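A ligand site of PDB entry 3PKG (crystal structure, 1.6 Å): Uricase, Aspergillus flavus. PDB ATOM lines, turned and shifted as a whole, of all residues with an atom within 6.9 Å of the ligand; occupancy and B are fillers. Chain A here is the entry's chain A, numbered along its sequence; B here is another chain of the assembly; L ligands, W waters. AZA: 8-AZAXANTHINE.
Water W1 lies within hydrogen-bond range of N9 of the ligand (2.7 Å) and NH1 of Arg 177 (3.4 Å). Water W2 lies within hydrogen-bond range of the side-chain hydroxyl (OG1) of Thr 58 of chain B and the side-chain amide nitrogen (ND2) of Asn 255.
Merely in contact with the ligand: Phe 160 (3.4 Å), Leu 171 (3.8 Å), Ser 227 (3.6 Å), Tyr 9 of chain B (3.8 Å), Ile 55 of chain B (3.6 Å), Ala 57 of chain B (3.5 Å) and Asp 59 of chain B (3.9 Å). Within 4 Å of the ligand: Phe 160, Leu 171, Arg 177, Ser 227, Val 228, Gln 229, Asn 255, Tyr 9 of chain B, Ile 55 of chain B, Ala 57 of chain B, Thr 58 of chain B and Asp 59 of chain B. Along chain A the residues within 4 Å of the ligand span positions 160 to 255.
The guanidinium group of Arg 177 is in hydrogen-bond range of an oxygen (O2) of the ligand (2.8 Å). N of Val 228 is in hydrogen-bond range of O2 of the ligand (2.9 Å). ND2 of Asn 255 lies close to N3 of the ligand, 3.3 Å away. N7 of the ligand lies within hydrogen-bond range of N of Thr 58 of chain B (2.8 Å). The side-chain hydroxyl of Thr 58 of chain B sits at hydrogen-bond distance from a nitrogen (N7) of the ligand (3.2 Å). The side-chain amide nitrogen of Gln 229 lies within hydrogen-bond range of an oxygen (O6) of the ligand (2.9 Å).
The backbone carbonyl oxygen (O) of Gly 287 is in hydrogen-bond range of the backbone NH (N) of Asn 255 (2.8 Å). N of Arg 177 lies within hydrogen-bond range of O of Ser 158. O of Asn 255 is in hydrogen-bond range of NE2 of His 257 (3.4 Å). The side-chain amino group of Lys 11 of chain B is in hydrogen-bond range of the side-chain hydroxyl of Thr 58 of chain B. The side-chain hydroxyl (OH) of Tyr 9 of chain B is in hydrogen-bond range of the backbone carbonyl oxygen (O) of Val 56 of chain B (2.6 Å). N of Ala 230 lies within hydrogen-bond range of OG of Ser 227. The backbone NH (N) of Gln 229 sits close to the side-chain hydroxyl (OG) of Ser 227, at 3.4 Å. The backbone carbonyl oxygen (O) of Ser 227 sits at hydrogen-bond distance from the side-chain hydroxyl (OG) of Ser 225 (2.9 Å).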
ATOM      1  N   SER A 158      11.731 -18.995  -2.595  1.00  0.00           N
ATOM      2  CA  SER A 158      11.113 -18.236  -3.669  1.00  0.00           C
ATOM      3  C   SER A 158      11.605 -16.807  -3.515  1.00  0.00           C
ATOM      4  O   SER A 158      11.644 -16.253  -2.397  1.00  0.00           O
ATOM      5  CB  SER A 158       9.583 -18.284  -3.573  1.00  0.00           C
ATOM      6  OG  SER A 158       8.990 -17.401  -4.497  1.00  0.00           O
ATOM      7  N   GLN A 159      11.959 -16.199  -4.636  1.00  0.00           N
ATOM      8  CA  GLN A 159      12.499 -14.852  -4.685  1.00  0.00           C
ATOM      9  C   GLN A 159      11.766 -14.061  -5.757  1.00  0.00           C
ATOM     10  O   GLN A 159      11.196 -14.638  -6.694  1.00  0.00           O
ATOM     11  CB  GLN A 159      14.005 -14.891  -5.056  1.00  0.00           C
ATOM     12  CG  GLN A 159      14.811 -15.835  -4.174  1.00  0.00           C
ATOM     13  CD  GLN A 159      16.303 -15.795  -4.468  1.00  0.00           C
ATOM     14  OE1 GLN A 159      16.778 -14.969  -5.233  1.00  0.00           O
ATOM     15  NE2 GLN A 159      17.041 -16.687  -3.822  1.00  0.00           N
ATOM     16  N   PHE A 160      11.819 -12.756  -5.642  1.00  0.00           N
ATOM     17  CA  PHE A 160      11.345 -11.900  -6.716  1.00  0.00           C
ATOM     18  C   PHE A 160      11.984 -10.532  -6.629  1.00  0.00           C
ATOM     19  O   PHE A 160      11.581  -9.690  -5.839  1.00  0.00           O
ATOM     20  CB  PHE A 160       9.799 -11.817  -6.755  1.00  0.00           C
ATOM     21  CG  PHE A 160       9.280 -11.189  -8.028  1.00  0.00           C
ATOM     22  CD1 PHE A 160       9.506 -11.804  -9.264  1.00  0.00           C
ATOM     23  CD2 PHE A 160       8.604  -9.963  -8.007  1.00  0.00           C
ATOM     24  CE1 PHE A 160       9.066 -11.216 -10.445  1.00  0.00           C
ATOM     25  CE2 PHE A 160       8.140  -9.383  -9.187  1.00  0.00           C
ATOM     26  CZ  PHE A 160       8.386 -10.005 -10.416  1.00  0.00           C
ATOM     27  N   PHE A 163      12.793  -6.662 -11.071  1.00  0.00           N
ATOM     28  CA  PHE A 163      11.722  -6.235 -11.971  1.00  0.00           C
ATOM     29  C   PHE A 163      11.755  -4.728 -12.277  1.00  0.00           C
ATOM     30  O   PHE A 163      12.437  -3.958 -11.592  1.00  0.00           O
ATOM     31  CB  PHE A 163      10.343  -6.641 -11.398  1.00  0.00           C
ATOM     32  CG  PHE A 163      10.148  -6.239  -9.965  1.00  0.00           C
ATOM     33  CD1 PHE A 163      10.537  -7.093  -8.945  1.00  0.00           C
ATOM     34  CD2 PHE A 163       9.566  -5.005  -9.638  1.00  0.00           C
ATOM     35  CE1 PHE A 163      10.365  -6.748  -7.593  1.00  0.00           C
ATOM     36  CE2 PHE A 163       9.385  -4.645  -8.300  1.00  0.00           C
ATOM     37  CZ  PHE A 163       9.791  -5.512  -7.286  1.00  0.00           C
ATOM     38  N   LEU A 171       6.136  -2.127  -4.962  1.00  0.00           N
ATOM     39  CA  LEU A 171       6.557  -3.448  -4.497  1.00  0.00           C
ATOM     40  C   LEU A 171       8.047  -3.486  -4.154  1.00  0.00           C
ATOM     41  O   LEU A 171       8.882  -3.078  -4.968  1.00  0.00           O
ATOM     42  CB  LEU A 171       6.274  -4.487  -5.590  1.00  0.00           C
ATOM     43  CG  LEU A 171       6.610  -5.951  -5.236  1.00  0.00           C
ATOM     44  CD1 LEU A 171       5.696  -6.477  -4.118  1.00  0.00           C
ATOM     45  CD2 LEU A 171       6.459  -6.818  -6.478  1.00  0.00           C
ATOM     46  N   ARG A 177      10.343 -15.311   0.057  1.00  0.00           N
ATOM     47  CA  ARG A 177       8.882 -15.096   0.191  1.00  0.00           C
ATOM     48  C   ARG A 177       8.181 -16.427   0.148  1.00  0.00           C
ATOM     49  O   ARG A 177       8.747 -17.446  -0.219  1.00  0.00           O
ATOM     50  CB  ARG A 177       8.353 -14.176  -0.919  1.00  0.00           C
ATOM     51  CG  ARG A 177       8.411 -14.835  -2.288  1.00  0.00           C
ATOM     52  CD  ARG A 177       7.905 -13.915  -3.380  1.00  0.00           C
ATOM     53  NE  ARG A 177       7.892 -14.633  -4.663  1.00  0.00           N
ATOM     54  CZ  ARG A 177       7.298 -14.204  -5.778  1.00  0.00           C
ATOM     55  NH1 ARG A 177       6.671 -13.020  -5.828  1.00  0.00           N
ATOM     56  NH2 ARG A 177       7.347 -14.963  -6.869  1.00  0.00           N
ATOM     57  N   LEU A 179       5.475 -18.834  -1.654  1.00  0.00           N
ATOM     58  CA  LEU A 179       4.898 -19.033  -2.990  1.00  0.00           C
ATOM     59  C   LEU A 179       3.802 -20.078  -2.934  1.00  0.00           C
ATOM     60  O   LEU A 179       4.012 -21.204  -2.512  1.00  0.00           O
ATOM     61  CB  LEU A 179       5.995 -19.419  -3.989  1.00  0.00           C
ATOM     62  CG  LEU A 179       5.574 -19.626  -5.437  1.00  0.00           C
ATOM     63  CD1 LEU A 179       4.968 -18.350  -6.030  1.00  0.00           C
ATOM     64  CD2 LEU A 179       6.795 -20.085  -6.266  1.00  0.00           C
ATOM     65  N   SER A 225      13.123 -20.506  -6.763  1.00  0.00           N
ATOM     66  CA  SER A 225      12.348 -19.866  -7.821  1.00  0.00           C
ATOM     67  C   SER A 225      12.690 -18.397  -7.968  1.00  0.00           C
ATOM     68  O   SER A 225      12.654 -17.629  -6.990  1.00  0.00           O
ATOM     69  CB  SER A 225      10.847 -20.056  -7.523  1.00  0.00           C
ATOM     70  OG  SER A 225      10.090 -19.300  -8.435  1.00  0.00           O
ATOM     71  N   ALA A 226      12.963 -17.983  -9.192  1.00  0.00           N
ATOM     72  CA  ALA A 226      13.283 -16.608  -9.495  1.00  0.00           C
ATOM     73  C   ALA A 226      12.026 -15.788  -9.777  1.00  0.00           C
ATOM     74  O   ALA A 226      12.054 -14.553  -9.775  1.00  0.00           O
ATOM     75  CB  ALA A 226      14.240 -16.564 -10.704  1.00  0.00           C
ATOM     76  N   SER A 227      10.948 -16.516 -10.062  1.00  0.00           N
ATOM     77  CA  SER A 227       9.632 -15.936 -10.387  1.00  0.00           C
ATOM     78  C   SER A 227       8.724 -17.094 -10.721  1.00  0.00           C
ATOM     79  O   SER A 227       9.190 -18.209 -10.984  1.00  0.00           O
ATOM     80  CB  SER A 227       9.673 -14.976 -11.598  1.00  0.00           C
ATOM     81  OG  SER A 227      10.027 -15.682 -12.793  1.00  0.00           O
ATOM     82  N   VAL A 228       7.410 -16.841 -10.752  1.00  0.00           N
ATOM     83  CA  VAL A 228       6.491 -17.871 -11.197  1.00  0.00           C
ATOM     84  C   VAL A 228       6.803 -18.225 -12.656  1.00  0.00           C
ATOM     85  O   VAL A 228       6.834 -19.409 -13.028  1.00  0.00           O
ATOM     86  CB  VAL A 228       5.022 -17.375 -11.040  1.00  0.00           C
ATOM     87  CG1 VAL A 228       4.043 -18.344 -11.664  1.00  0.00           C
ATOM     88  CG2 VAL A 228       4.733 -17.195  -9.523  1.00  0.00           C
ATOM     89  N   GLN A 229       7.060 -17.197 -13.466  1.00  0.00           N
ATOM     90  CA  GLN A 229       7.405 -17.340 -14.894  1.00  0.00           C
ATOM     91  C   GLN A 229       8.543 -18.339 -15.093  1.00  0.00           C
ATOM     92  O   GLN A 229       8.433 -19.274 -15.906  1.00  0.00           O
ATOM     93  CB  GLN A 229       7.836 -15.991 -15.469  1.00  0.00           C
ATOM     94  CG  GLN A 229       6.660 -15.003 -15.683  1.00  0.00           C
ATOM     95  CD  GLN A 229       6.324 -14.134 -14.477  1.00  0.00           C
ATOM     96  OE1 GLN A 229       6.555 -14.492 -13.324  1.00  0.00           O
ATOM     97  NE2 GLN A 229       5.722 -12.967 -14.767  1.00  0.00           N
ATOM     98  N   ALA A 230       9.624 -18.158 -14.339  1.00  0.00           N
ATOM     99  CA  ALA A 230      10.799 -19.000 -14.553  1.00  0.00           C
ATOM    100  C   ALA A 230      10.577 -20.452 -14.111  1.00  0.00           C
ATOM    101  O   ALA A 230      10.994 -21.409 -14.799  1.00  0.00           O
ATOM    102  CB  ALA A 230      12.006 -18.385 -13.852  1.00  0.00           C
ATOM    103  N   ASN A 255      -0.909 -16.372  -8.544  1.00  0.00           N
ATOM    104  CA  ASN A 255       0.056 -16.153  -7.509  1.00  0.00           C
ATOM    105  C   ASN A 255      -0.768 -15.734  -6.273  1.00  0.00           C
ATOM    106  O   ASN A 255      -1.264 -14.616  -6.246  1.00  0.00           O
ATOM    107  CB  ASN A 255       1.050 -15.071  -7.988  1.00  0.00           C
ATOM    108  CG  ASN A 255       2.227 -14.920  -7.070  1.00  0.00           C
ATOM    109  OD1 ASN A 255       2.364 -15.659  -6.084  1.00  0.00           O
ATOM    110  ND2 ASN A 255       3.116 -13.962  -7.375  1.00  0.00           N
ATOM    111  N   HIS A 257      -1.211 -14.501  -2.819  1.00  0.00           N
ATOM    112  CA  HIS A 257      -0.272 -13.741  -1.993  1.00  0.00           C
ATOM    113  C   HIS A 257      -0.502 -13.926  -0.507  1.00  0.00           C
ATOM    114  O   HIS A 257      -1.645 -13.976  -0.037  1.00  0.00           O
ATOM    115  CB  HIS A 257      -0.335 -12.249  -2.326  1.00  0.00           C
ATOM    116  CG  HIS A 257      -0.203 -11.940  -3.795  1.00  0.00           C
ATOM    117  ND1 HIS A 257       0.955 -12.170  -4.499  1.00  0.00           N
ATOM    118  CD2 HIS A 257      -1.089 -11.431  -4.682  1.00  0.00           C
ATOM    119  CE1 HIS A 257       0.786 -11.795  -5.756  1.00  0.00           C
ATOM    120  NE2 HIS A 257      -0.450 -11.354  -5.892  1.00  0.00           N
ATOM    121  N   GLY A 287      -2.022 -12.385  -8.619  1.00  0.00           N
ATOM    122  CA  GLY A 287      -1.318 -12.492  -9.895  1.00  0.00           C
ATOM    123  C   GLY A 287      -1.860 -13.646 -10.711  1.00  0.00           C
ATOM    124  O   GLY A 287      -2.381 -14.619 -10.159  1.00  0.00           O
ATOM    125  N   ILE A 289      -0.476 -15.831 -14.124  1.00  0.00           N
ATOM    126  CA  ILE A 289       0.657 -15.969 -15.023  1.00  0.00           C
ATOM    127  C   ILE A 289       0.400 -17.156 -15.926  1.00  0.00           C
ATOM    128  O   ILE A 289       0.083 -18.247 -15.434  1.00  0.00           O
ATOM    129  CB  ILE A 289       1.966 -16.232 -14.210  1.00  0.00           C
ATOM    130  CG1 ILE A 289       2.071 -15.318 -12.949  1.00  0.00           C
ATOM    131  CG2 ILE A 289       3.187 -16.101 -15.159  1.00  0.00           C
ATOM    132  CD1 ILE A 289       2.127 -13.886 -13.198  1.00  0.00           C
ATOM    133  N   TYR B   9       0.473 -12.293 -18.713  1.00  0.00           N
ATOM    134  CA  TYR B   9       0.523 -12.340 -17.247  1.00  0.00           C
ATOM    135  C   TYR B   9      -0.059 -11.004 -16.761  1.00  0.00           C
ATOM    136  O   TYR B   9      -0.076 -10.025 -17.509  1.00  0.00           O
ATOM    137  CB  TYR B   9       1.964 -12.567 -16.756  1.00  0.00           C
ATOM    138  CG  TYR B   9       2.719 -11.270 -16.716  1.00  0.00           C
ATOM    139  CD1 TYR B   9       3.129 -10.656 -17.902  1.00  0.00           C
ATOM    140  CD2 TYR B   9       2.946 -10.596 -15.516  1.00  0.00           C
ATOM    141  CE1 TYR B   9       3.760  -9.402 -17.892  1.00  0.00           C
ATOM    142  CE2 TYR B   9       3.567  -9.359 -15.480  1.00  0.00           C
ATOM    143  CZ  TYR B   9       3.968  -8.772 -16.682  1.00  0.00           C
ATOM    144  OH  TYR B   9       4.584  -7.548 -16.670  1.00  0.00           O
ATOM    145  N   GLY B  10      -0.529 -10.979 -15.520  1.00  0.00           N
ATOM    146  CA  GLY B  10      -1.063  -9.739 -14.982  1.00  0.00           C
ATOM    147  C   GLY B  10      -1.736  -9.940 -13.646  1.00  0.00           C
ATOM    148  O   GLY B  10      -1.343 -10.789 -12.871  1.00  0.00           O
ATOM    149  N   LYS B  11      -2.767  -9.141 -13.369  1.00  0.00           N
ATOM    150  CA  LYS B  11      -3.444  -9.170 -12.063  1.00  0.00           C
ATOM    151  C   LYS B  11      -4.910  -9.460 -12.287  1.00  0.00           C
ATOM    152  O   LYS B  11      -5.533  -8.851 -13.171  1.00  0.00           O
ATOM    153  CB  LYS B  11      -3.306  -7.832 -11.321  1.00  0.00           C
ATOM    154  CG  LYS B  11      -3.489  -7.947  -9.800  1.00  0.00           C
ATOM    155  CD  LYS B  11      -2.342  -8.767  -9.195  1.00  0.00           C
ATOM    156  CE  LYS B  11      -1.760  -8.178  -7.952  1.00  0.00           C
ATOM    157  NZ  LYS B  11      -0.503  -8.894  -7.554  1.00  0.00           N
ATOM    158  N   ASN B  52      14.004 -10.745 -14.977  1.00  0.00           N
ATOM    159  CA  ASN B  52      12.858  -9.981 -14.479  1.00  0.00           C
ATOM    160  C   ASN B  52      12.793  -8.534 -14.967  1.00  0.00           C
ATOM    161  O   ASN B  52      11.822  -7.838 -14.709  1.00  0.00           O
ATOM    162  CB  ASN B  52      12.730 -10.067 -12.945  1.00  0.00           C
ATOM    163  CG  ASN B  52      12.393 -11.477 -12.457  1.00  0.00           C
ATOM    164  OD1 ASN B  52      11.846 -12.288 -13.202  1.00  0.00           O
ATOM    165  ND2 ASN B  52      12.733 -11.775 -11.214  1.00  0.00           N
ATOM    166  N   ILE B  55       9.675  -7.426 -16.691  1.00  0.00           N
ATOM    167  CA  ILE B  55       8.398  -7.582 -15.991  1.00  0.00           C
ATOM    168  C   ILE B  55       7.913  -6.301 -15.323  1.00  0.00           C
ATOM    169  O   ILE B  55       8.586  -5.766 -14.436  1.00  0.00           O
ATOM    170  CB  ILE B  55       8.437  -8.706 -14.926  1.00  0.00           C
ATOM    171  CG1 ILE B  55       8.691 -10.076 -15.562  1.00  0.00           C
ATOM    172  CG2 ILE B  55       7.065  -8.759 -14.136  1.00  0.00           C
ATOM    173  CD1 ILE B  55       7.624 -10.491 -16.589  1.00  0.00           C
ATOM    174  N   VAL B  56       6.764  -5.811 -15.785  1.00  0.00           N
ATOM    175  CA  VAL B  56       5.994  -4.813 -15.047  1.00  0.00           C
ATOM    176  C   VAL B  56       5.306  -5.635 -13.944  1.00  0.00           C
ATOM    177  O   VAL B  56       4.499  -6.508 -14.267  1.00  0.00           O
ATOM    178  CB  VAL B  56       4.980  -4.127 -15.978  1.00  0.00           C
ATOM    179  CG1 VAL B  56       4.076  -3.149 -15.207  1.00  0.00           C
ATOM    180  CG2 VAL B  56       5.748  -3.386 -17.090  1.00  0.00           C
ATOM    181  N   ALA B  57       5.660  -5.402 -12.680  1.00  0.00           N
ATOM    182  CA  ALA B  57       5.154  -6.281 -11.598  1.00  0.00           C
ATOM    183  C   ALA B  57       3.628  -6.259 -11.570  1.00  0.00           C
ATOM    184  O   ALA B  57       3.017  -5.227 -11.853  1.00  0.00           O
ATOM    185  CB  ALA B  57       5.742  -5.893 -10.230  1.00  0.00           C
ATOM    186  N   THR B  58       3.038  -7.403 -11.231  1.00  0.00           N
ATOM    187  CA  THR B  58       1.571  -7.479 -11.200  1.00  0.00           C
ATOM    188  C   THR B  58       1.053  -6.527 -10.132  1.00  0.00           C
ATOM    189  O   THR B  58      -0.010  -5.929 -10.305  1.00  0.00           O
ATOM    190  CB  THR B  58       1.046  -8.909 -10.991  1.00  0.00           C
ATOM    191  OG1 THR B  58       1.398  -9.360  -9.681  1.00  0.00           O
ATOM    192  CG2 THR B  58       1.643  -9.852 -12.049  1.00  0.00           C
ATOM    193  N   ASP B  59       1.835  -6.358  -9.053  1.00  0.00           N
ATOM    194  CA  ASP B  59       1.514  -5.355  -8.024  1.00  0.00           C
ATOM    195  C   ASP B  59       1.393  -3.945  -8.601  1.00  0.00           C
ATOM    196  O   ASP B  59       0.503  -3.178  -8.219  1.00  0.00           O
ATOM    197  CB  ASP B  59       2.541  -5.403  -6.892  1.00  0.00           C
ATOM    198  CG  ASP B  59       2.106  -4.586  -5.685  1.00  0.00           C
ATOM    199  OD1 ASP B  59       1.298  -5.099  -4.881  1.00  0.00           O
ATOM    200  OD2 ASP B  59       2.567  -3.434  -5.546  1.00  0.00           O
ATOM    201  N   SER B  60       2.297  -3.604  -9.535  1.00  0.00           N
ATOM    202  CA  SER B  60       2.247  -2.303 -10.235  1.00  0.00           C
ATOM    203  C   SER B  60       1.038  -2.171 -11.150  1.00  0.00           C
ATOM    204  O   SER B  60       0.474  -1.083 -11.302  1.00  0.00           O
ATOM    205  CB  SER B  60       3.544  -2.082 -11.028  1.00  0.00           C
ATOM    206  OG  SER B  60       4.615  -2.267 -10.127  1.00  0.00           O
HETATM  207  N1  AZA L   1       5.851 -12.820 -10.985  1.00  0.00           N
HETATM  208  C2  AZA L   1       6.079 -13.202  -9.705  1.00  0.00           C
HETATM  209  O2  AZA L   1       6.540 -14.337  -9.521  1.00  0.00           O
HETATM  210  N3  AZA L   1       5.782 -12.415  -8.621  1.00  0.00           N
HETATM  211  C4  AZA L   1       5.318 -11.181  -8.894  1.00  0.00           C
HETATM  212  C5  AZA L   1       5.075 -10.711 -10.215  1.00  0.00           C
HETATM  213  C6  AZA L   1       5.383 -11.623 -11.327  1.00  0.00           C
HETATM  214  O6  AZA L   1       5.159 -11.278 -12.501  1.00  0.00           O
HETATM  215  N7  AZA L   1       4.584  -9.430 -10.182  1.00  0.00           N
HETATM  216  N8  AZA L   1       4.537  -9.168  -8.801  1.00  0.00           N
HETATM  217  N9  AZA L   1       4.967 -10.220  -7.966  1.00  0.00           N
HETATM  218  O   HOH W   1       4.636 -10.392  -5.292  1.00  0.00           O
HETATM  219  O   HOH W   2       1.958 -12.048  -9.198  1.00  0.00           O
